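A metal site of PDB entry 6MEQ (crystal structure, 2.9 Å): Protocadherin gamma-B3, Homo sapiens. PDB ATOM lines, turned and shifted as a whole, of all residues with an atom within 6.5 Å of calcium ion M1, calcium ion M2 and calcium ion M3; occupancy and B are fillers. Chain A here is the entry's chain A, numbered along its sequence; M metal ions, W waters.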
ATOM      1  N   GLU A 223      -1.665 -27.694  -5.784  1.00  0.00           N
ATOM      2  CA  GLU A 223      -1.823 -26.348  -5.239  1.00  0.00           C
ATOM      3  C   GLU A 223      -3.176 -26.184  -4.574  1.00  0.00           C
ATOM      4  O   GLU A 223      -3.266 -25.821  -3.393  1.00  0.00           O
ATOM      5  CB  GLU A 223      -1.644 -25.311  -6.355  1.00  0.00           C
ATOM      6  CG  GLU A 223      -1.513 -23.881  -5.856  1.00  0.00           C
ATOM      7  CD  GLU A 223      -1.634 -22.866  -6.970  1.00  0.00           C
ATOM      8  OE1 GLU A 223      -2.666 -22.156  -7.015  1.00  0.00           O
ATOM      9  OE2 GLU A 223      -0.705 -22.772  -7.796  1.00  0.00           O
ATOM     10  N   ASN A 224      -4.255 -26.444  -5.308  1.00  0.00           N
ATOM     11  CA  ASN A 224      -5.612 -26.302  -4.782  1.00  0.00           C
ATOM     12  C   ASN A 224      -6.083 -27.605  -4.140  1.00  0.00           C
ATOM     13  O   ASN A 224      -7.093 -28.203  -4.521  1.00  0.00           O
ATOM     14  CB  ASN A 224      -6.562 -25.834  -5.881  1.00  0.00           C
ATOM     15  CG  ASN A 224      -6.208 -24.468  -6.421  1.00  0.00           C
ATOM     16  OD1 ASN A 224      -5.671 -23.622  -5.706  1.00  0.00           O
ATOM     17  ND2 ASN A 224      -6.502 -24.241  -7.698  1.00  0.00           N
ATOM     18  N   LEU A 277      -3.777 -24.112   0.476  1.00  0.00           N
ATOM     19  CA  LEU A 277      -2.431 -24.018  -0.052  1.00  0.00           C
ATOM     20  C   LEU A 277      -2.404 -23.074  -1.256  1.00  0.00           C
ATOM     21  O   LEU A 277      -3.383 -22.941  -1.980  1.00  0.00           O
ATOM     22  CB  LEU A 277      -1.919 -25.403  -0.465  1.00  0.00           C
ATOM     23  CG  LEU A 277      -1.899 -26.478   0.614  1.00  0.00           C
ATOM     24  CD1 LEU A 277      -1.362 -27.791   0.061  1.00  0.00           C
ATOM     25  CD2 LEU A 277      -1.078 -26.021   1.812  1.00  0.00           C
ATOM     26  N   ASP A 278      -1.259 -22.422  -1.447  1.00  0.00           N
ATOM     27  CA  ASP A 278      -1.100 -21.472  -2.542  1.00  0.00           C
ATOM     28  C   ASP A 278       0.349 -21.472  -2.990  1.00  0.00           C
ATOM     29  O   ASP A 278       1.250 -21.178  -2.188  1.00  0.00           O
ATOM     30  CB  ASP A 278      -1.530 -20.062  -2.107  1.00  0.00           C
ATOM     31  CG  ASP A 278      -1.643 -19.102  -3.280  1.00  0.00           C
ATOM     32  OD1 ASP A 278      -1.502 -19.551  -4.433  1.00  0.00           O
ATOM     33  OD2 ASP A 278      -1.858 -17.898  -3.039  1.00  0.00           O
ATOM     34  N   PHE A 279       0.577 -21.815  -4.262  1.00  0.00           N
ATOM     35  CA  PHE A 279       1.943 -21.843  -4.784  1.00  0.00           C
ATOM     36  C   PHE A 279       2.517 -20.447  -4.936  1.00  0.00           C
ATOM     37  O   PHE A 279       3.732 -20.255  -4.765  1.00  0.00           O
ATOM     38  CB  PHE A 279       1.959 -22.582  -6.123  1.00  0.00           C
ATOM     39  CG  PHE A 279       3.324 -22.685  -6.750  1.00  0.00           C
ATOM     40  CD1 PHE A 279       4.174 -23.722  -6.420  1.00  0.00           C
ATOM     41  CD2 PHE A 279       3.748 -21.746  -7.676  1.00  0.00           C
ATOM     42  CE1 PHE A 279       5.430 -23.824  -6.994  1.00  0.00           C
ATOM     43  CE2 PHE A 279       5.004 -21.838  -8.251  1.00  0.00           C
ATOM     44  CZ  PHE A 279       5.844 -22.872  -7.912  1.00  0.00           C
ATOM     45  N   GLU A 280       1.677 -19.462  -5.264  1.00  0.00           N
ATOM     46  CA  GLU A 280       2.160 -18.092  -5.439  1.00  0.00           C
ATOM     47  C   GLU A 280       2.624 -17.461  -4.139  1.00  0.00           C
ATOM     48  O   GLU A 280       3.362 -16.477  -4.169  1.00  0.00           O
ATOM     49  CB  GLU A 280       1.072 -17.233  -6.081  1.00  0.00           C
ATOM     50  CG  GLU A 280       0.903 -17.436  -7.580  1.00  0.00           C
ATOM     51  CD  GLU A 280       0.316 -18.783  -7.931  1.00  0.00           C
ATOM     52  OE1 GLU A 280      -0.391 -19.372  -7.079  1.00  0.00           O
ATOM     53  OE2 GLU A 280       0.557 -19.267  -9.058  1.00  0.00           O
ATOM     54  N   SER A 308       3.061 -28.092  -6.020  1.00  0.00           N
ATOM     55  CA  SER A 308       3.153 -27.878  -7.457  1.00  0.00           C
ATOM     56  C   SER A 308       2.210 -26.763  -7.885  1.00  0.00           C
ATOM     57  O   SER A 308       1.155 -26.562  -7.289  1.00  0.00           O
ATOM     58  CB  SER A 308       2.835 -29.165  -8.220  1.00  0.00           C
ATOM     59  OG  SER A 308       1.533 -29.628  -7.915  1.00  0.00           O
ATOM     60  N   ASP A 309       2.591 -26.059  -8.940  1.00  0.00           N
ATOM     61  CA  ASP A 309       1.807 -24.935  -9.426  1.00  0.00           C
ATOM     62  C   ASP A 309       0.635 -25.406 -10.272  1.00  0.00           C
ATOM     63  O   ASP A 309       0.784 -26.297 -11.118  1.00  0.00           O
ATOM     64  CB  ASP A 309       2.684 -23.978 -10.244  1.00  0.00           C
ATOM     65  CG  ASP A 309       1.897 -22.825 -10.828  1.00  0.00           C
ATOM     66  OD1 ASP A 309       1.405 -21.984 -10.055  1.00  0.00           O
ATOM     67  OD2 ASP A 309       1.784 -22.754 -12.074  1.00  0.00           O
ATOM     68  N   GLU A 310      -0.531 -24.807 -10.042  1.00  0.00           N
ATOM     69  CA  GLU A 310      -1.721 -25.078 -10.821  1.00  0.00           C
ATOM     70  C   GLU A 310      -2.162 -23.811 -11.543  1.00  0.00           C
ATOM     71  O   GLU A 310      -1.961 -22.702 -11.055  1.00  0.00           O
ATOM     72  CB  GLU A 310      -2.877 -25.591  -9.934  1.00  0.00           C
ATOM     73  CG  GLU A 310      -2.671 -26.993  -9.390  1.00  0.00           C
ATOM     74  CD  GLU A 310      -2.807 -28.072 -10.462  1.00  0.00           C
ATOM     75  OE1 GLU A 310      -3.366 -27.769 -11.533  1.00  0.00           O
ATOM     76  OE2 GLU A 310      -2.369 -29.214 -10.220  1.00  0.00           O
ATOM     77  N   ASN A 311      -2.743 -23.996 -12.728  1.00  0.00           N
ATOM     78  CA  ASN A 311      -3.206 -22.875 -13.549  1.00  0.00           C
ATOM     79  C   ASN A 311      -4.574 -22.428 -13.032  1.00  0.00           C
ATOM     80  O   ASN A 311      -5.628 -22.776 -13.571  1.00  0.00           O
ATOM     81  CB  ASN A 311      -3.254 -23.266 -15.018  1.00  0.00           C
ATOM     82  CG  ASN A 311      -3.660 -22.112 -15.921  1.00  0.00           C
ATOM     83  OD1 ASN A 311      -3.492 -20.949 -15.557  1.00  0.00           O
ATOM     84  ND2 ASN A 311      -4.190 -22.435 -17.085  1.00  0.00           N
ATOM     85  N   ASP A 312      -4.547 -21.628 -11.965  1.00  0.00           N
ATOM     86  CA  ASP A 312      -5.763 -21.099 -11.367  1.00  0.00           C
ATOM     87  C   ASP A 312      -5.806 -19.570 -11.411  1.00  0.00           C
ATOM     88  O   ASP A 312      -6.671 -18.974 -10.756  1.00  0.00           O
ATOM     89  CB  ASP A 312      -5.904 -21.577  -9.919  1.00  0.00           C
ATOM     90  CG  ASP A 312      -4.781 -21.076  -9.027  1.00  0.00           C
ATOM     91  OD1 ASP A 312      -3.654 -20.913  -9.514  1.00  0.00           O
ATOM     92  OD2 ASP A 312      -5.050 -20.841  -7.821  1.00  0.00           O
ATOM     93  N   ASN A 313      -4.927 -18.937 -12.165  1.00  0.00           N
ATOM     94  CA  ASN A 313      -4.903 -17.485 -12.325  1.00  0.00           C
ATOM     95  C   ASN A 313      -5.102 -17.136 -13.787  1.00  0.00           C
ATOM     96  O   ASN A 313      -4.414 -17.682 -14.664  1.00  0.00           O
ATOM     97  CB  ASN A 313      -3.590 -16.894 -11.808  1.00  0.00           C
ATOM     98  CG  ASN A 313      -3.511 -16.874 -10.295  1.00  0.00           C
ATOM     99  OD1 ASN A 313      -3.906 -15.908  -9.656  1.00  0.00           O
ATOM    100  ND2 ASN A 313      -2.994 -17.958  -9.720  1.00  0.00           N
ATOM    101  N   ALA A 314      -6.041 -16.230 -14.054  1.00  0.00           N
ATOM    102  CA  ALA A 314      -6.337 -15.785 -15.411  1.00  0.00           C
ATOM    103  C   ALA A 314      -5.409 -14.639 -15.812  1.00  0.00           C
ATOM    104  O   ALA A 314      -4.978 -13.847 -14.969  1.00  0.00           O
ATOM    105  CB  ALA A 314      -7.781 -15.329 -15.520  1.00  0.00           C
ATOM    106  N   PRO A 315      -5.073 -14.543 -17.096  1.00  0.00           N
ATOM    107  CA  PRO A 315      -4.216 -13.430 -17.549  1.00  0.00           C
ATOM    108  C   PRO A 315      -4.903 -12.095 -17.346  1.00  0.00           C
ATOM    109  O   PRO A 315      -6.109 -11.942 -17.535  1.00  0.00           O
ATOM    110  CB  PRO A 315      -4.005 -13.729 -19.036  1.00  0.00           C
ATOM    111  CG  PRO A 315      -4.276 -15.202 -19.182  1.00  0.00           C
ATOM    112  CD  PRO A 315      -5.350 -15.503 -18.181  1.00  0.00           C
ATOM    113  N   ASP A 343       0.803 -12.791 -15.701  1.00  0.00           N
ATOM    114  CA  ASP A 343       0.071 -13.883 -15.071  1.00  0.00           C
ATOM    115  C   ASP A 343       0.814 -14.318 -13.820  1.00  0.00           C
ATOM    116  O   ASP A 343       2.045 -14.474 -13.826  1.00  0.00           O
ATOM    117  CB  ASP A 343      -0.083 -15.071 -16.035  1.00  0.00           C
ATOM    118  CG  ASP A 343      -1.160 -16.043 -15.588  1.00  0.00           C
ATOM    119  OD1 ASP A 343      -2.355 -15.745 -15.770  1.00  0.00           O
ATOM    120  OD2 ASP A 343      -0.804 -17.116 -15.042  1.00  0.00           O
ATOM    121  N   LEU A 344       0.063 -14.525 -12.736  1.00  0.00           N
ATOM    122  CA  LEU A 344       0.667 -14.861 -11.453  1.00  0.00           C
ATOM    123  C   LEU A 344       1.250 -16.270 -11.440  1.00  0.00           C
ATOM    124  O   LEU A 344       2.113 -16.563 -10.605  1.00  0.00           O
ATOM    125  CB  LEU A 344      -0.354 -14.701 -10.324  1.00  0.00           C
ATOM    126  CG  LEU A 344      -0.921 -13.296 -10.130  1.00  0.00           C
ATOM    127  CD1 LEU A 344      -1.881 -13.258  -8.954  1.00  0.00           C
ATOM    128  CD2 LEU A 344       0.202 -12.281  -9.952  1.00  0.00           C
ATOM    129  N   ASP A 345       0.798 -17.144 -12.326  1.00  0.00           N
ATOM    130  CA  ASP A 345       1.290 -18.512 -12.351  1.00  0.00           C
ATOM    131  C   ASP A 345       2.705 -18.555 -12.943  1.00  0.00           C
ATOM    132  O   ASP A 345       3.209 -17.581 -13.499  1.00  0.00           O
ATOM    133  CB  ASP A 345       0.350 -19.412 -13.156  1.00  0.00           C
ATOM    134  CG  ASP A 345      -1.077 -19.355 -12.640  1.00  0.00           C
ATOM    135  OD1 ASP A 345      -1.265 -19.320 -11.411  1.00  0.00           O
ATOM    136  OD2 ASP A 345      -2.009 -19.348 -13.469  1.00  0.00           O
ATOM    137  N   SER A 346       3.340 -19.723 -12.823  1.00  0.00           N
ATOM    138  CA  SER A 346       4.698 -19.934 -13.292  1.00  0.00           C
ATOM    139  C   SER A 346       4.710 -20.944 -14.425  1.00  0.00           C
ATOM    140  O   SER A 346       3.703 -21.589 -14.743  1.00  0.00           O
ATOM    141  CB  SER A 346       5.600 -20.410 -12.138  1.00  0.00           C
ATOM    142  OG  SER A 346       5.616 -19.459 -11.085  1.00  0.00           O
ATOM    143  N   PHE A 348       4.708 -22.653 -18.055  1.00  0.00           N
ATOM    144  CA  PHE A 348       3.847 -22.412 -19.207  1.00  0.00           C
ATOM    145  C   PHE A 348       2.487 -21.855 -18.797  1.00  0.00           C
ATOM    146  O   PHE A 348       1.773 -21.307 -19.644  1.00  0.00           O
ATOM    147  CB  PHE A 348       3.658 -23.697 -20.015  1.00  0.00           C
ATOM    148  CG  PHE A 348       4.815 -24.019 -20.915  1.00  0.00           C
ATOM    149  CD1 PHE A 348       4.881 -23.491 -22.188  1.00  0.00           C
ATOM    150  CD2 PHE A 348       5.828 -24.855 -20.481  1.00  0.00           C
ATOM    151  CE1 PHE A 348       5.940 -23.787 -23.019  1.00  0.00           C
ATOM    152  CE2 PHE A 348       6.897 -25.152 -21.313  1.00  0.00           C
ATOM    153  CZ  PHE A 348       6.953 -24.614 -22.588  1.00  0.00           C
ATOM    154  N   ASN A 349       2.120 -21.974 -17.518  1.00  0.00           N
ATOM    155  CA  ASN A 349       0.871 -21.400 -17.033  1.00  0.00           C
ATOM    156  C   ASN A 349       0.931 -19.880 -16.944  1.00  0.00           C
ATOM    157  O   ASN A 349      -0.126 -19.246 -16.786  1.00  0.00           O
ATOM    158  CB  ASN A 349       0.518 -21.981 -15.669  1.00  0.00           C
ATOM    159  CG  ASN A 349       0.420 -23.494 -15.687  1.00  0.00           C
ATOM    160  OD1 ASN A 349       0.054 -24.090 -16.700  1.00  0.00           O
ATOM    161  ND2 ASN A 349       0.731 -24.114 -14.556  1.00  0.00           N
ATOM    162  N   GLY A 350       2.118 -19.280 -17.051  1.00  0.00           N
ATOM    163  CA  GLY A 350       2.247 -17.843 -17.006  1.00  0.00           C
ATOM    164  C   GLY A 350       2.480 -17.220 -18.367  1.00  0.00           C
ATOM    165  O   GLY A 350       2.324 -15.997 -18.532  1.00  0.00           O
ATOM    166  N   GLU A 351       2.866 -18.029 -19.351  1.00  0.00           N
ATOM    167  CA  GLU A 351       3.070 -17.538 -20.701  1.00  0.00           C
ATOM    168  C   GLU A 351       1.733 -17.111 -21.299  1.00  0.00           C
ATOM    169  O   GLU A 351       0.792 -17.907 -21.379  1.00  0.00           O
ATOM    170  CB  GLU A 351       3.719 -18.625 -21.566  1.00  0.00           C
ATOM    171  CG  GLU A 351       5.006 -19.190 -20.986  1.00  0.00           C
ATOM    172  CD  GLU A 351       6.135 -18.173 -20.973  1.00  0.00           C
ATOM    173  OE1 GLU A 351       6.122 -17.248 -21.812  1.00  0.00           O
ATOM    174  OE2 GLU A 351       7.028 -18.306 -20.113  1.00  0.00           O
ATOM    175  N   ASP A 396      -3.515 -17.871 -21.573  1.00  0.00           N
ATOM    176  CA  ASP A 396      -2.291 -18.516 -21.117  1.00  0.00           C
ATOM    177  C   ASP A 396      -2.127 -19.864 -21.806  1.00  0.00           C
ATOM    178  O   ASP A 396      -2.967 -20.307 -22.586  1.00  0.00           O
ATOM    179  CB  ASP A 396      -2.311 -18.668 -19.593  1.00  0.00           C
ATOM    180  CG  ASP A 396      -3.507 -19.443 -19.086  1.00  0.00           C
ATOM    181  OD1 ASP A 396      -3.540 -20.674 -19.263  1.00  0.00           O
ATOM    182  OD2 ASP A 396      -4.423 -18.814 -18.509  1.00  0.00           O
ATOM    183  N   LYS A 397      -1.008 -20.538 -21.516  1.00  0.00           N
ATOM    184  CA  LYS A 397      -0.681 -21.830 -22.099  1.00  0.00           C
ATOM    185  C   LYS A 397      -0.782 -22.948 -21.068  1.00  0.00           C
ATOM    186  O   LYS A 397       0.050 -23.867 -21.032  1.00  0.00           O
ATOM    187  CB  LYS A 397       0.723 -21.807 -22.715  1.00  0.00           C
ATOM    188  CG  LYS A 397       0.924 -20.735 -23.768  1.00  0.00           C
ATOM    189  CD  LYS A 397       2.351 -20.728 -24.279  1.00  0.00           C
ATOM    190  CE  LYS A 397       2.573 -19.618 -25.300  1.00  0.00           C
ATOM    191  NZ  LYS A 397       1.721 -19.788 -26.502  1.00  0.00           N
ATOM    192  N   GLY A 398      -1.811 -22.894 -20.223  1.00  0.00           N
ATOM    193  CA  GLY A 398      -2.012 -23.879 -19.190  1.00  0.00           C
ATOM    194  C   GLY A 398      -2.972 -24.988 -19.607  1.00  0.00           C
ATOM    195  O   GLY A 398      -3.461 -25.036 -20.733  1.00  0.00           O
ATOM    196  N   LEU A 402      -6.780 -20.589 -19.230  1.00  0.00           N
ATOM    197  CA  LEU A 402      -7.692 -19.525 -18.856  1.00  0.00           C
ATOM    198  C   LEU A 402      -7.499 -18.333 -19.793  1.00  0.00           C
ATOM    199  O   LEU A 402      -6.497 -18.220 -20.492  1.00  0.00           O
ATOM    200  CB  LEU A 402      -7.485 -19.095 -17.400  1.00  0.00           C
ATOM    201  CG  LEU A 402      -8.034 -19.992 -16.286  1.00  0.00           C
ATOM    202  CD1 LEU A 402      -7.208 -21.260 -16.118  1.00  0.00           C
ATOM    203  CD2 LEU A 402      -8.101 -19.218 -14.974  1.00  0.00           C
HETATM  204 CA    CA M   1      -2.508 -18.593 -16.053  1.00  0.00          CA
HETATM  205 CA    CA M   2      -1.171 -21.001  -9.445  1.00  0.00          CA
HETATM  206 CA    CA M   3      -3.160 -19.895  -6.271  1.00  0.00          CA
HETATM  207  O   HOH W   1      -5.701 -17.793  -7.265  1.00  0.00           O
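The backbone NH (N) of Glu 223 lies close to the backbone carbonyl oxygen (O) of Ser 308 (3.4 Å). The backbone NH (N) of Glu 280 lies close to the side-chain carboxylate (OD1) of Asp 278, 3.3 Å away. The side-chain carboxylate (OD1) of Asp 312 lies close to the side-chain amide nitrogen (ND2) of Asn 313, at 3.0 Å. The side-chain amide nitrogen (ND2) of Asn 349 sits at hydrogen-bond distance from the side-chain carboxylate (OD2) of Asp 309 (3.0 Å). The side-chain amide nitrogen of Asn 311 is in hydrogen-bond range of the side-chain carboxylate of Asp 396. N of Ser 346 sits at hydrogen-bond distance from OD2 of Asp 309. The side-chain carboxylate (OD2) of Asp 396 sits at hydrogen-bond distance from the backbone NH (N) of Leu 402. The side-chain carboxylate (OD1) of Asp 396 is in hydrogen-bond range of the backbone NH (N) of Gly 398 (3.0 Å).
Six residues have an atom within 4 Å of calcium ion M1: Asn 311, Asn 313, Asp 343, Asp 345, Asn 349 and Asp 396. Along chain A the residues within 4 Å of calcium ion M1 span positions 311 to 396. The nearest printed residue that does not touch calcium ion M1 is Ala 314 (4.7 Å).
Of the 26 residues printed, 7 come within 4 Å of calcium ion M2. The nearest printed residue that does not touch calcium ion M2 is Asn 311 (4.7 Å).
Within 4 Å of calcium ion M3: Glu 223, Asp 278, Glu 280, Asp 312 and Asn 313.
OD2 of Asp 343 binds calcium ion M1 (2.5 Å). The backbone carbonyl oxygen (O) of Asn 313 is bound to calcium ion M1. Calcium ion M1 is bound by O of Asn 349. OD1 of Asn 311 is bound to calcium ion M1 (2.6 Å). OD2 of Asp 345 is bound to calcium ion M1. The side-chain carboxylate (OD1) of Asp 343 is bound to calcium ion M1 (2.9 Å). Slightly farther from calcium ion M1 lies the side-chain carboxylate (OD2) of Asp 396 (3.1 Å).
OE2 of Glu 223 is bound to calcium ion M2, 2.5 Å away. Calcium ion M2 is bound by O of Glu 310. Calcium ion M2 is bound by OE2 of Glu 280 (2.5 Å). Calcium ion M2 is bound by OD1 of Asp 312, 2.5 Å away. The side-chain carboxylate (OD1) of Asp 345 is bound to calcium ion M2, at 2.6 Å. The side-chain carboxylate (OD1) of Asp 309 is bound to calcium ion M2 (2.8 Å). Calcium ion M2 has six donor atoms within binding distance. Slightly farther from calcium ion M2 lies the side-chain carboxylate (OE1) of Glu 280 (3.0 Å). Slightly farther from calcium ion M2 lies OE1 of Glu 223 (3.1 Å).
Calcium ion M3 is bound by OE1 of Glu 223, OD1 of Asp 278 and OD2 of Asp 312. Slightly farther from calcium ion M3 lies the side-chain carboxylate (OE1) of Glu 280 (2.9 Å).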
